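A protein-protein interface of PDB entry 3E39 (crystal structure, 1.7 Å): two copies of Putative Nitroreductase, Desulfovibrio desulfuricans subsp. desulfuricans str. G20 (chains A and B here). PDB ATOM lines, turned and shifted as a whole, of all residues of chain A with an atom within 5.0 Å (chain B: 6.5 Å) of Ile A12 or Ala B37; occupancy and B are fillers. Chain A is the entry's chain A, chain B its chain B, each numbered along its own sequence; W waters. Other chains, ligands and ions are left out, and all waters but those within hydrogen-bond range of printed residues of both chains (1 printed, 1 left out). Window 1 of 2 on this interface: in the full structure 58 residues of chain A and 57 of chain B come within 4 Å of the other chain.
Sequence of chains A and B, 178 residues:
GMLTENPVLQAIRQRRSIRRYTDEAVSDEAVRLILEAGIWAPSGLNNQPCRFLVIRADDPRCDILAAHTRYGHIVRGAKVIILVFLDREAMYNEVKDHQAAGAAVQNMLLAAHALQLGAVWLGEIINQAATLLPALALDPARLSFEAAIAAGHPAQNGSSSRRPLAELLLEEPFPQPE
Ile A12 touches just these residues of chain B: Ala B37 and Asn B107.
Printed residues of chain B within 4 Å of Arg A15: Trp B40.
Ala B37 touches one residue of chain A.
Of the printed residues of chain A, Asn B107 touches Ile A12 and Leu A110.
Of the printed residues of chain A, Ala B111 touches Leu A9.
The nearest residue of chain B that does not touch Ile A12 is Trp B40 (4.05 Å).
The nearest residue of chain A that does not touch Ala B37 is Leu A9 (4.9 Å).
The guanidinium group (NH2) of Arg A15 is in hydrogen-bond range of the backbone carbonyl oxygen (O) of Trp B40 (3.3 Å).
Leu A110 touches Val B8, but with the chains exchanged Val A8 does not touch Leu B110 (4.1 Å).
Leu A110 touches its own counterpart, Leu B110.
2 positions are printed for both chains.
Of the 10 pairs that touch across the chains among the printed residues, 1 has its exchanged pair printed and touching as well.
The backbone carbonyl oxygen of Ala B37 is in hydrogen-bond range of the side-chain amide nitrogen of Asn B107 (3.0 Å).
The side-chain amide nitrogen (ND2) of Asn B107 sits close to the backbone NH (N) of Ala B41 (3.3 Å).
Hydrophobic or aromatic side chains of chain A that line the printed part of chain B: Val A8, Leu A9, Ala A11, Ile A12 and Leu A110.
Printed residues of chain B that touch a printed residue of chain A: Val B8, Ala B37, Trp B40, Asn B107, Leu B110, Ala B111 and Ala B114.
Among the printed residues, 10 pairs touch across the chains.
Among the printed residues, no Asp or Glu carboxylate lies within 4 Å of a Lys or Arg side-chain nitrogen of the other chain.
Among the printed residues, pairs that only touch across the chains: Arg A13 with Trp B40 (3.2 Å), Ile A12 with Asn B107 (3.4 Å), Leu A110 with Leu B110 (3.4 Å), Leu A9 with Ala B111 (3.5 Å), Ile A12 with Ala B37 (3.5 Å), Leu A110 with Asn B107 (3.6 Å), Val A8 with Ala B114 (3.7 Å), Ala A11 with Val B8 (3.7 Å) and Leu A110 with Val B8 (3.95 Å).
Water W1 lies within hydrogen-bond range of O of Trp B40, O of Ile A12, NE of Arg A15 and ND2 of Asn B107.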
ATOM      1  N   VAL A   8      23.059   2.772 -15.844  1.00  0.00           N
ATOM      2  CA  VAL A   8      22.233   2.997 -14.646  1.00  0.00           C
ATOM      3  C   VAL A   8      20.940   2.211 -14.808  1.00  0.00           C
ATOM      4  O   VAL A   8      20.539   1.468 -13.893  1.00  0.00           O
ATOM      5  CB  VAL A   8      21.972   4.504 -14.364  1.00  0.00           C
ATOM      6  CG1 VAL A   8      21.048   4.660 -13.210  1.00  0.00           C
ATOM      7  CG2 VAL A   8      23.293   5.249 -14.120  1.00  0.00           C
ATOM      8  N   LEU A   9      20.276   2.314 -15.960  1.00  0.00           N
ATOM      9  CA  LEU A   9      19.080   1.480 -16.173  1.00  0.00           C
ATOM     10  C   LEU A   9      19.393  -0.030 -16.101  1.00  0.00           C
ATOM     11  O   LEU A   9      18.627  -0.788 -15.510  1.00  0.00           O
ATOM     12  CB  LEU A   9      18.368   1.855 -17.479  1.00  0.00           C
ATOM     13  CG  LEU A   9      17.938   3.338 -17.601  1.00  0.00           C
ATOM     14  CD1 LEU A   9      17.268   3.654 -18.951  1.00  0.00           C
ATOM     15  CD2 LEU A   9      17.021   3.749 -16.456  1.00  0.00           C
ATOM     16  N   GLN A  10      20.530  -0.460 -16.658  1.00  0.00           N
ATOM     17  CA  GLN A  10      20.925  -1.877 -16.594  1.00  0.00           C
ATOM     18  C   GLN A  10      21.106  -2.331 -15.147  1.00  0.00           C
ATOM     19  O   GLN A  10      20.584  -3.386 -14.739  1.00  0.00           O
ATOM     20  CB  GLN A  10      22.228  -2.126 -17.373  1.00  0.00           C
ATOM     21  CG  GLN A  10      22.074  -2.005 -18.872  1.00  0.00           C
ATOM     22  CD  GLN A  10      23.395  -2.083 -19.608  1.00  0.00           C
ATOM     23  OE1 GLN A  10      24.414  -2.513 -19.047  1.00  0.00           O
ATOM     24  NE2 GLN A  10      23.389  -1.664 -20.886  1.00  0.00           N
ATOM     25  N   ALA A  11      21.777  -1.499 -14.343  1.00  0.00           N
ATOM     26  CA  ALA A  11      22.016  -1.834 -12.918  1.00  0.00           C
ATOM     27  C   ALA A  11      20.694  -2.019 -12.161  1.00  0.00           C
ATOM     28  O   ALA A  11      20.514  -2.961 -11.379  1.00  0.00           O
ATOM     29  CB  ALA A  11      22.870  -0.737 -12.233  1.00  0.00           C
ATOM     30  N   ILE A  12      19.756  -1.102 -12.400  1.00  0.00           N
ATOM     31  CA  ILE A  12      18.440  -1.174 -11.767  1.00  0.00           C
ATOM     32  C   ILE A  12      17.761  -2.480 -12.113  1.00  0.00           C
ATOM     33  O   ILE A  12      17.196  -3.120 -11.259  1.00  0.00           O
ATOM     34  CB  ILE A  12      17.571   0.053 -12.132  1.00  0.00           C
ATOM     35  CG1 ILE A  12      18.161   1.263 -11.430  1.00  0.00           C
ATOM     36  CG2 ILE A  12      16.100  -0.166 -11.750  1.00  0.00           C
ATOM     37  CD1 ILE A  12      17.745   2.620 -11.951  1.00  0.00           C
ATOM     38  N   ARG A  13      17.858  -2.898 -13.368  1.00  0.00           N
ATOM     39  CA  ARG A  13      17.179  -4.107 -13.790  1.00  0.00           C
ATOM     40  C   ARG A  13      17.888  -5.412 -13.396  1.00  0.00           C
ATOM     41  O   ARG A  13      17.221  -6.407 -13.111  1.00  0.00           O
ATOM     42  CB  ARG A  13      17.002  -4.045 -15.315  1.00  0.00           C
ATOM     43  CG  ARG A  13      16.448  -5.304 -15.996  1.00  0.00           C
ATOM     44  CD  ARG A  13      15.076  -5.709 -15.495  1.00  0.00           C
ATOM     45  NE  ARG A  13      14.582  -6.920 -16.142  1.00  0.00           N
ATOM     46  CZ  ARG A  13      14.920  -8.154 -15.781  1.00  0.00           C
ATOM     47  NH1 ARG A  13      15.750  -8.353 -14.774  1.00  0.00           N
ATOM     48  NH2 ARG A  13      14.421  -9.202 -16.438  1.00  0.00           N
ATOM     49  N   GLN A  14      19.207  -5.366 -13.391  1.00  0.00           N
ATOM     50  CA  GLN A  14      20.044  -6.541 -13.171  1.00  0.00           C
ATOM     51  C   GLN A  14      20.493  -6.767 -11.726  1.00  0.00           C
ATOM     52  O   GLN A  14      20.959  -7.840 -11.380  1.00  0.00           O
ATOM     53  CB  GLN A  14      21.223  -6.466 -14.124  1.00  0.00           C
ATOM     54  CG  GLN A  14      20.787  -6.625 -15.584  1.00  0.00           C
ATOM     55  CD  GLN A  14      21.798  -6.122 -16.574  1.00  0.00           C
ATOM     56  OE1 GLN A  14      22.895  -5.714 -16.205  1.00  0.00           O
ATOM     57  NE2 GLN A  14      21.420  -6.120 -17.858  1.00  0.00           N
ATOM     58  N   ARG A  15      20.341  -5.761 -10.877  1.00  0.00           N
ATOM     59  CA  ARG A  15      20.627  -5.940  -9.463  1.00  0.00           C
ATOM     60  C   ARG A  15      19.780  -7.087  -8.925  1.00  0.00           C
ATOM     61  O   ARG A  15      18.550  -7.077  -9.055  1.00  0.00           O
ATOM     62  CB  ARG A  15      20.226  -4.702  -8.687  1.00  0.00           C
ATOM     63  CG  ARG A  15      20.345  -4.834  -7.153  1.00  0.00           C
ATOM     64  CD  ARG A  15      19.204  -4.057  -6.403  1.00  0.00           C
ATOM     65  NE  ARG A  15      17.889  -4.479  -6.905  1.00  0.00           N
ATOM     66  CZ  ARG A  15      17.211  -5.543  -6.484  1.00  0.00           C
ATOM     67  NH1 ARG A  15      17.718  -6.346  -5.546  1.00  0.00           N
ATOM     68  NH2 ARG A  15      16.057  -5.843  -7.050  1.00  0.00           N
ATOM     69  N   LEU A 110      22.457  -0.897  -5.198  1.00  0.00           N
ATOM     70  CA  LEU A 110      22.897  -0.520  -6.540  1.00  0.00           C
ATOM     71  C   LEU A 110      24.424  -0.275  -6.544  1.00  0.00           C
ATOM     72  O   LEU A 110      25.144  -0.694  -7.455  1.00  0.00           O
ATOM     73  CB  LEU A 110      22.141   0.713  -7.040  1.00  0.00           C
ATOM     74  CG  LEU A 110      20.652   0.472  -7.338  1.00  0.00           C
ATOM     75  CD1 LEU A 110      19.902   1.781  -7.660  1.00  0.00           C
ATOM     76  CD2 LEU A 110      20.488  -0.548  -8.499  1.00  0.00           C
ATOM     77  N   VAL B   8      27.117   4.396 -12.279  1.00  0.00           N
ATOM     78  CA  VAL B   8      26.062   4.171 -11.276  1.00  0.00           C
ATOM     79  C   VAL B   8      26.374   4.989 -10.006  1.00  0.00           C
ATOM     80  O   VAL B   8      25.508   5.691  -9.430  1.00  0.00           O
ATOM     81  CB  VAL B   8      25.904   2.674 -10.959  1.00  0.00           C
ATOM     82  CG1 VAL B   8      24.901   2.453  -9.830  1.00  0.00           C
ATOM     83  CG2 VAL B   8      25.480   1.873 -12.223  1.00  0.00           C
ATOM     84  N   ARG B  32       7.988   5.253 -19.705  1.00  0.00           N
ATOM     85  CA  ARG B  32       7.950   3.820 -19.571  1.00  0.00           C
ATOM     86  C   ARG B  32       9.239   3.327 -18.889  1.00  0.00           C
ATOM     87  O   ARG B  32       9.187   2.471 -18.000  1.00  0.00           O
ATOM     88  CB  ARG B  32       7.732   3.133 -20.925  1.00  0.00           C
ATOM     89  CG  ARG B  32       7.458   1.622 -20.827  1.00  0.00           C
ATOM     90  CD  ARG B  32       7.501   0.953 -22.180  1.00  0.00           C
ATOM     91  NE  ARG B  32       8.858   0.993 -22.720  1.00  0.00           N
ATOM     92  CZ  ARG B  32       9.831   0.152 -22.348  1.00  0.00           C
ATOM     93  NH1 ARG B  32       9.600  -0.811 -21.450  1.00  0.00           N
ATOM     94  NH2 ARG B  32      11.035   0.260 -22.882  1.00  0.00           N
ATOM     95  N   LEU B  33      10.385   3.875 -19.309  1.00  0.00           N
ATOM     96  CA  LEU B  33      11.662   3.456 -18.746  1.00  0.00           C
ATOM     97  C   LEU B  33      11.746   3.756 -17.260  1.00  0.00           C
ATOM     98  O   LEU B  33      12.220   2.932 -16.484  1.00  0.00           O
ATOM     99  CB  LEU B  33      12.809   4.081 -19.511  1.00  0.00           C
ATOM    100  CG  LEU B  33      13.028   3.533 -20.936  1.00  0.00           C
ATOM    101  CD1 LEU B  33      13.953   4.452 -21.754  1.00  0.00           C
ATOM    102  CD2 LEU B  33      13.544   2.100 -20.886  1.00  0.00           C
ATOM    103  N   ILE B  34      11.265   4.933 -16.869  1.00  0.00           N
ATOM    104  CA  ILE B  34      11.239   5.315 -15.456  1.00  0.00           C
ATOM    105  C   ILE B  34      10.364   4.334 -14.661  1.00  0.00           C
ATOM    106  O   ILE B  34      10.790   3.830 -13.616  1.00  0.00           O
ATOM    107  CB  ILE B  34      10.766   6.775 -15.269  1.00  0.00           C
ATOM    108  CG1 ILE B  34      11.842   7.723 -15.816  1.00  0.00           C
ATOM    109  CG2 ILE B  34      10.550   7.087 -13.781  1.00  0.00           C
ATOM    110  CD1 ILE B  34      11.396   9.200 -15.915  1.00  0.00           C
ATOM    111  N   LEU B  35       9.166   4.044 -15.180  1.00  0.00           N
ATOM    112  CA  LEU B  35       8.235   3.099 -14.551  1.00  0.00           C
ATOM    113  C   LEU B  35       8.854   1.717 -14.409  1.00  0.00           C
ATOM    114  O   LEU B  35       8.755   1.102 -13.357  1.00  0.00           O
ATOM    115  CB  LEU B  35       6.918   3.026 -15.331  1.00  0.00           C
ATOM    116  CG  LEU B  35       6.008   4.253 -15.141  1.00  0.00           C
ATOM    117  CD1 LEU B  35       4.921   4.282 -16.218  1.00  0.00           C
ATOM    118  CD2 LEU B  35       5.376   4.374 -13.722  1.00  0.00           C
ATOM    119  N   GLU B  36       9.519   1.261 -15.464  1.00  0.00           N
ATOM    120  CA  GLU B  36      10.228  -0.027 -15.431  1.00  0.00           C
ATOM    121  C   GLU B  36      11.271  -0.068 -14.311  1.00  0.00           C
ATOM    122  O   GLU B  36      11.418  -1.075 -13.630  1.00  0.00           O
ATOM    123  CB  GLU B  36      10.888  -0.342 -16.764  1.00  0.00           C
ATOM    124  CG  GLU B  36       9.928  -0.823 -17.834  1.00  0.00           C
ATOM    125  CD  GLU B  36       9.425  -2.231 -17.585  1.00  0.00           C
ATOM    126  OE1 GLU B  36      10.198  -3.083 -17.100  1.00  0.00           O
ATOM    127  OE2 GLU B  36       8.252  -2.498 -17.878  1.00  0.00           O
ATOM    128  N   ALA B  37      12.006   1.021 -14.139  1.00  0.00           N
ATOM    129  CA  ALA B  37      12.969   1.124 -13.049  1.00  0.00           C
ATOM    130  C   ALA B  37      12.246   0.940 -11.707  1.00  0.00           C
ATOM    131  O   ALA B  37      12.725   0.236 -10.840  1.00  0.00           O
ATOM    132  CB  ALA B  37      13.683   2.470 -13.094  1.00  0.00           C
ATOM    133  N   GLY B  38      11.089   1.579 -11.555  1.00  0.00           N
ATOM    134  CA  GLY B  38      10.296   1.475 -10.341  1.00  0.00           C
ATOM    135  C   GLY B  38       9.853   0.065  -9.994  1.00  0.00           C
ATOM    136  O   GLY B  38      10.007  -0.385  -8.850  1.00  0.00           O
ATOM    137  N   ILE B  39       9.341  -0.660 -10.985  1.00  0.00           N
ATOM    138  CA  ILE B  39       8.792  -1.998 -10.721  1.00  0.00           C
ATOM    139  C   ILE B  39       9.866  -3.021 -10.368  1.00  0.00           C
ATOM    140  O   ILE B  39       9.559  -4.047  -9.741  1.00  0.00           O
ATOM    141  CB  ILE B  39       7.880  -2.501 -11.861  1.00  0.00           C
ATOM    142  CG1 ILE B  39       8.681  -2.878 -13.094  1.00  0.00           C
ATOM    143  CG2 ILE B  39       6.785  -1.449 -12.208  1.00  0.00           C
ATOM    144  CD1 ILE B  39       7.788  -3.434 -14.211  1.00  0.00           C
ATOM    145  N   TRP B  40      11.108  -2.757 -10.773  1.00  0.00           N
ATOM    146  CA  TRP B  40      12.229  -3.627 -10.468  1.00  0.00           C
ATOM    147  C   TRP B  40      12.922  -3.334  -9.118  1.00  0.00           C
ATOM    148  O   TRP B  40      13.871  -4.013  -8.743  1.00  0.00           O
ATOM    149  CB  TRP B  40      13.212  -3.715 -11.635  1.00  0.00           C
ATOM    150  CG  TRP B  40      12.704  -4.686 -12.678  1.00  0.00           C
ATOM    151  CD1 TRP B  40      11.991  -4.382 -13.799  1.00  0.00           C
ATOM    152  CD2 TRP B  40      12.858  -6.113 -12.670  1.00  0.00           C
ATOM    153  NE1 TRP B  40      11.685  -5.537 -14.492  1.00  0.00           N
ATOM    154  CE2 TRP B  40      12.206  -6.611 -13.819  1.00  0.00           C
ATOM    155  CE3 TRP B  40      13.484  -7.018 -11.806  1.00  0.00           C
ATOM    156  CZ2 TRP B  40      12.150  -7.974 -14.110  1.00  0.00           C
ATOM    157  CZ3 TRP B  40      13.418  -8.361 -12.088  1.00  0.00           C
ATOM    158  CH2 TRP B  40      12.755  -8.831 -13.227  1.00  0.00           C
ATOM    159  N   ALA B  41      12.410  -2.371  -8.360  1.00  0.00           N
ATOM    160  CA  ALA B  41      12.897  -2.210  -6.996  1.00  0.00           C
ATOM    161  C   ALA B  41      12.473  -3.525  -6.289  1.00  0.00           C
ATOM    162  O   ALA B  41      11.463  -4.168  -6.668  1.00  0.00           O
ATOM    163  CB  ALA B  41      12.262  -0.973  -6.299  1.00  0.00           C
ATOM    164  N   ALA B 103      12.323   2.529  -2.114  1.00  0.00           N
ATOM    165  CA  ALA B 103      13.272   1.924  -3.051  1.00  0.00           C
ATOM    166  C   ALA B 103      12.794   2.128  -4.511  1.00  0.00           C
ATOM    167  O   ALA B 103      13.577   2.430  -5.411  1.00  0.00           O
ATOM    168  CB  ALA B 103      13.491   0.459  -2.705  1.00  0.00           C
ATOM    169  N   ALA B 104      11.490   1.985  -4.732  1.00  0.00           N
ATOM    170  CA  ALA B 104      10.862   2.218  -6.050  1.00  0.00           C
ATOM    171  C   ALA B 104      11.023   3.653  -6.522  1.00  0.00           C
ATOM    172  O   ALA B 104      11.414   3.899  -7.669  1.00  0.00           O
ATOM    173  CB  ALA B 104       9.382   1.831  -5.986  1.00  0.00           C
ATOM    174  N   GLN B 106      13.242   5.787  -5.405  1.00  0.00           N
ATOM    175  CA  GLN B 106      14.657   6.027  -5.651  1.00  0.00           C
ATOM    176  C   GLN B 106      15.062   5.492  -7.025  1.00  0.00           C
ATOM    177  O   GLN B 106      15.762   6.163  -7.761  1.00  0.00           O
ATOM    178  CB  GLN B 106      15.530   5.426  -4.551  1.00  0.00           C
ATOM    179  CG  GLN B 106      17.012   5.803  -4.640  1.00  0.00           C
ATOM    180  CD  GLN B 106      17.278   7.315  -4.580  1.00  0.00           C
ATOM    181  OE1 GLN B 106      16.418   8.092  -4.178  1.00  0.00           O
ATOM    182  NE2 GLN B 106      18.501   7.726  -4.944  1.00  0.00           N
ATOM    183  N   ASN B 107      14.671   4.280  -7.368  1.00  0.00           N
ATOM    184  CA  ASN B 107      14.963   3.776  -8.718  1.00  0.00           C
ATOM    185  C   ASN B 107      14.457   4.717  -9.808  1.00  0.00           C
ATOM    186  O   ASN B 107      15.108   4.929 -10.841  1.00  0.00           O
ATOM    187  CB  ASN B 107      14.352   2.382  -8.960  1.00  0.00           C
ATOM    188  CG  ASN B 107      15.230   1.247  -8.488  1.00  0.00           C
ATOM    189  OD1 ASN B 107      16.345   1.450  -8.009  1.00  0.00           O
ATOM    190  ND2 ASN B 107      14.715   0.010  -8.621  1.00  0.00           N
ATOM    191  N   MET B 108      13.254   5.247  -9.615  1.00  0.00           N
ATOM    192  CA  MET B 108      12.676   6.160 -10.595  1.00  0.00           C
ATOM    193  C   MET B 108      13.414   7.480 -10.703  1.00  0.00           C
ATOM    194  O   MET B 108      13.553   8.010 -11.790  1.00  0.00           O
ATOM    195  CB  MET B 108      11.193   6.368 -10.330  1.00  0.00           C
ATOM    196  CG  MET B 108      10.435   5.121 -10.768  1.00  0.00           C
ATOM    197  SD  MET B 108       8.515   5.200 -10.734  1.00  0.00           S
ATOM    198  CE  MET B 108       8.592   5.114  -9.050  1.00  0.00           C
ATOM    199  N   LEU B 110      16.624   7.868  -9.999  1.00  0.00           N
ATOM    200  CA  LEU B 110      17.899   7.554 -10.641  1.00  0.00           C
ATOM    201  C   LEU B 110      17.735   7.370 -12.142  1.00  0.00           C
ATOM    202  O   LEU B 110      18.547   7.859 -12.926  1.00  0.00           O
ATOM    203  CB  LEU B 110      18.550   6.311 -10.018  1.00  0.00           C
ATOM    204  CG  LEU B 110      18.983   6.498  -8.563  1.00  0.00           C
ATOM    205  CD1 LEU B 110      19.319   5.171  -7.893  1.00  0.00           C
ATOM    206  CD2 LEU B 110      20.151   7.475  -8.435  1.00  0.00           C
ATOM    207  N   ALA B 111      16.709   6.622 -12.532  1.00  0.00           N
ATOM    208  CA  ALA B 111      16.376   6.420 -13.960  1.00  0.00           C
ATOM    209  C   ALA B 111      16.099   7.750 -14.661  1.00  0.00           C
ATOM    210  O   ALA B 111      16.573   7.982 -15.791  1.00  0.00           O
ATOM    211  CB  ALA B 111      15.180   5.532 -14.054  1.00  0.00           C
ATOM    212  N   ALA B 112      15.357   8.652 -13.996  1.00  0.00           N
ATOM    213  CA  ALA B 112      15.047   9.969 -14.597  1.00  0.00           C
ATOM    214  C   ALA B 112      16.384  10.684 -14.853  1.00  0.00           C
ATOM    215  O   ALA B 112      16.648  11.208 -15.957  1.00  0.00           O
ATOM    216  CB  ALA B 112      14.122  10.836 -13.700  1.00  0.00           C
ATOM    217  N   ALA B 114      19.323   9.366 -15.143  1.00  0.00           N
ATOM    218  CA  ALA B 114      20.071   8.639 -16.196  1.00  0.00           C
ATOM    219  C   ALA B 114      19.599   8.997 -17.618  1.00  0.00           C
ATOM    220  O   ALA B 114      20.357   8.856 -18.595  1.00  0.00           O
ATOM    221  CB  ALA B 114      19.984   7.129 -15.970  1.00  0.00           C
HETATM  222  O   HOH W   1      16.233  -2.680  -8.585  1.00  0.00           O
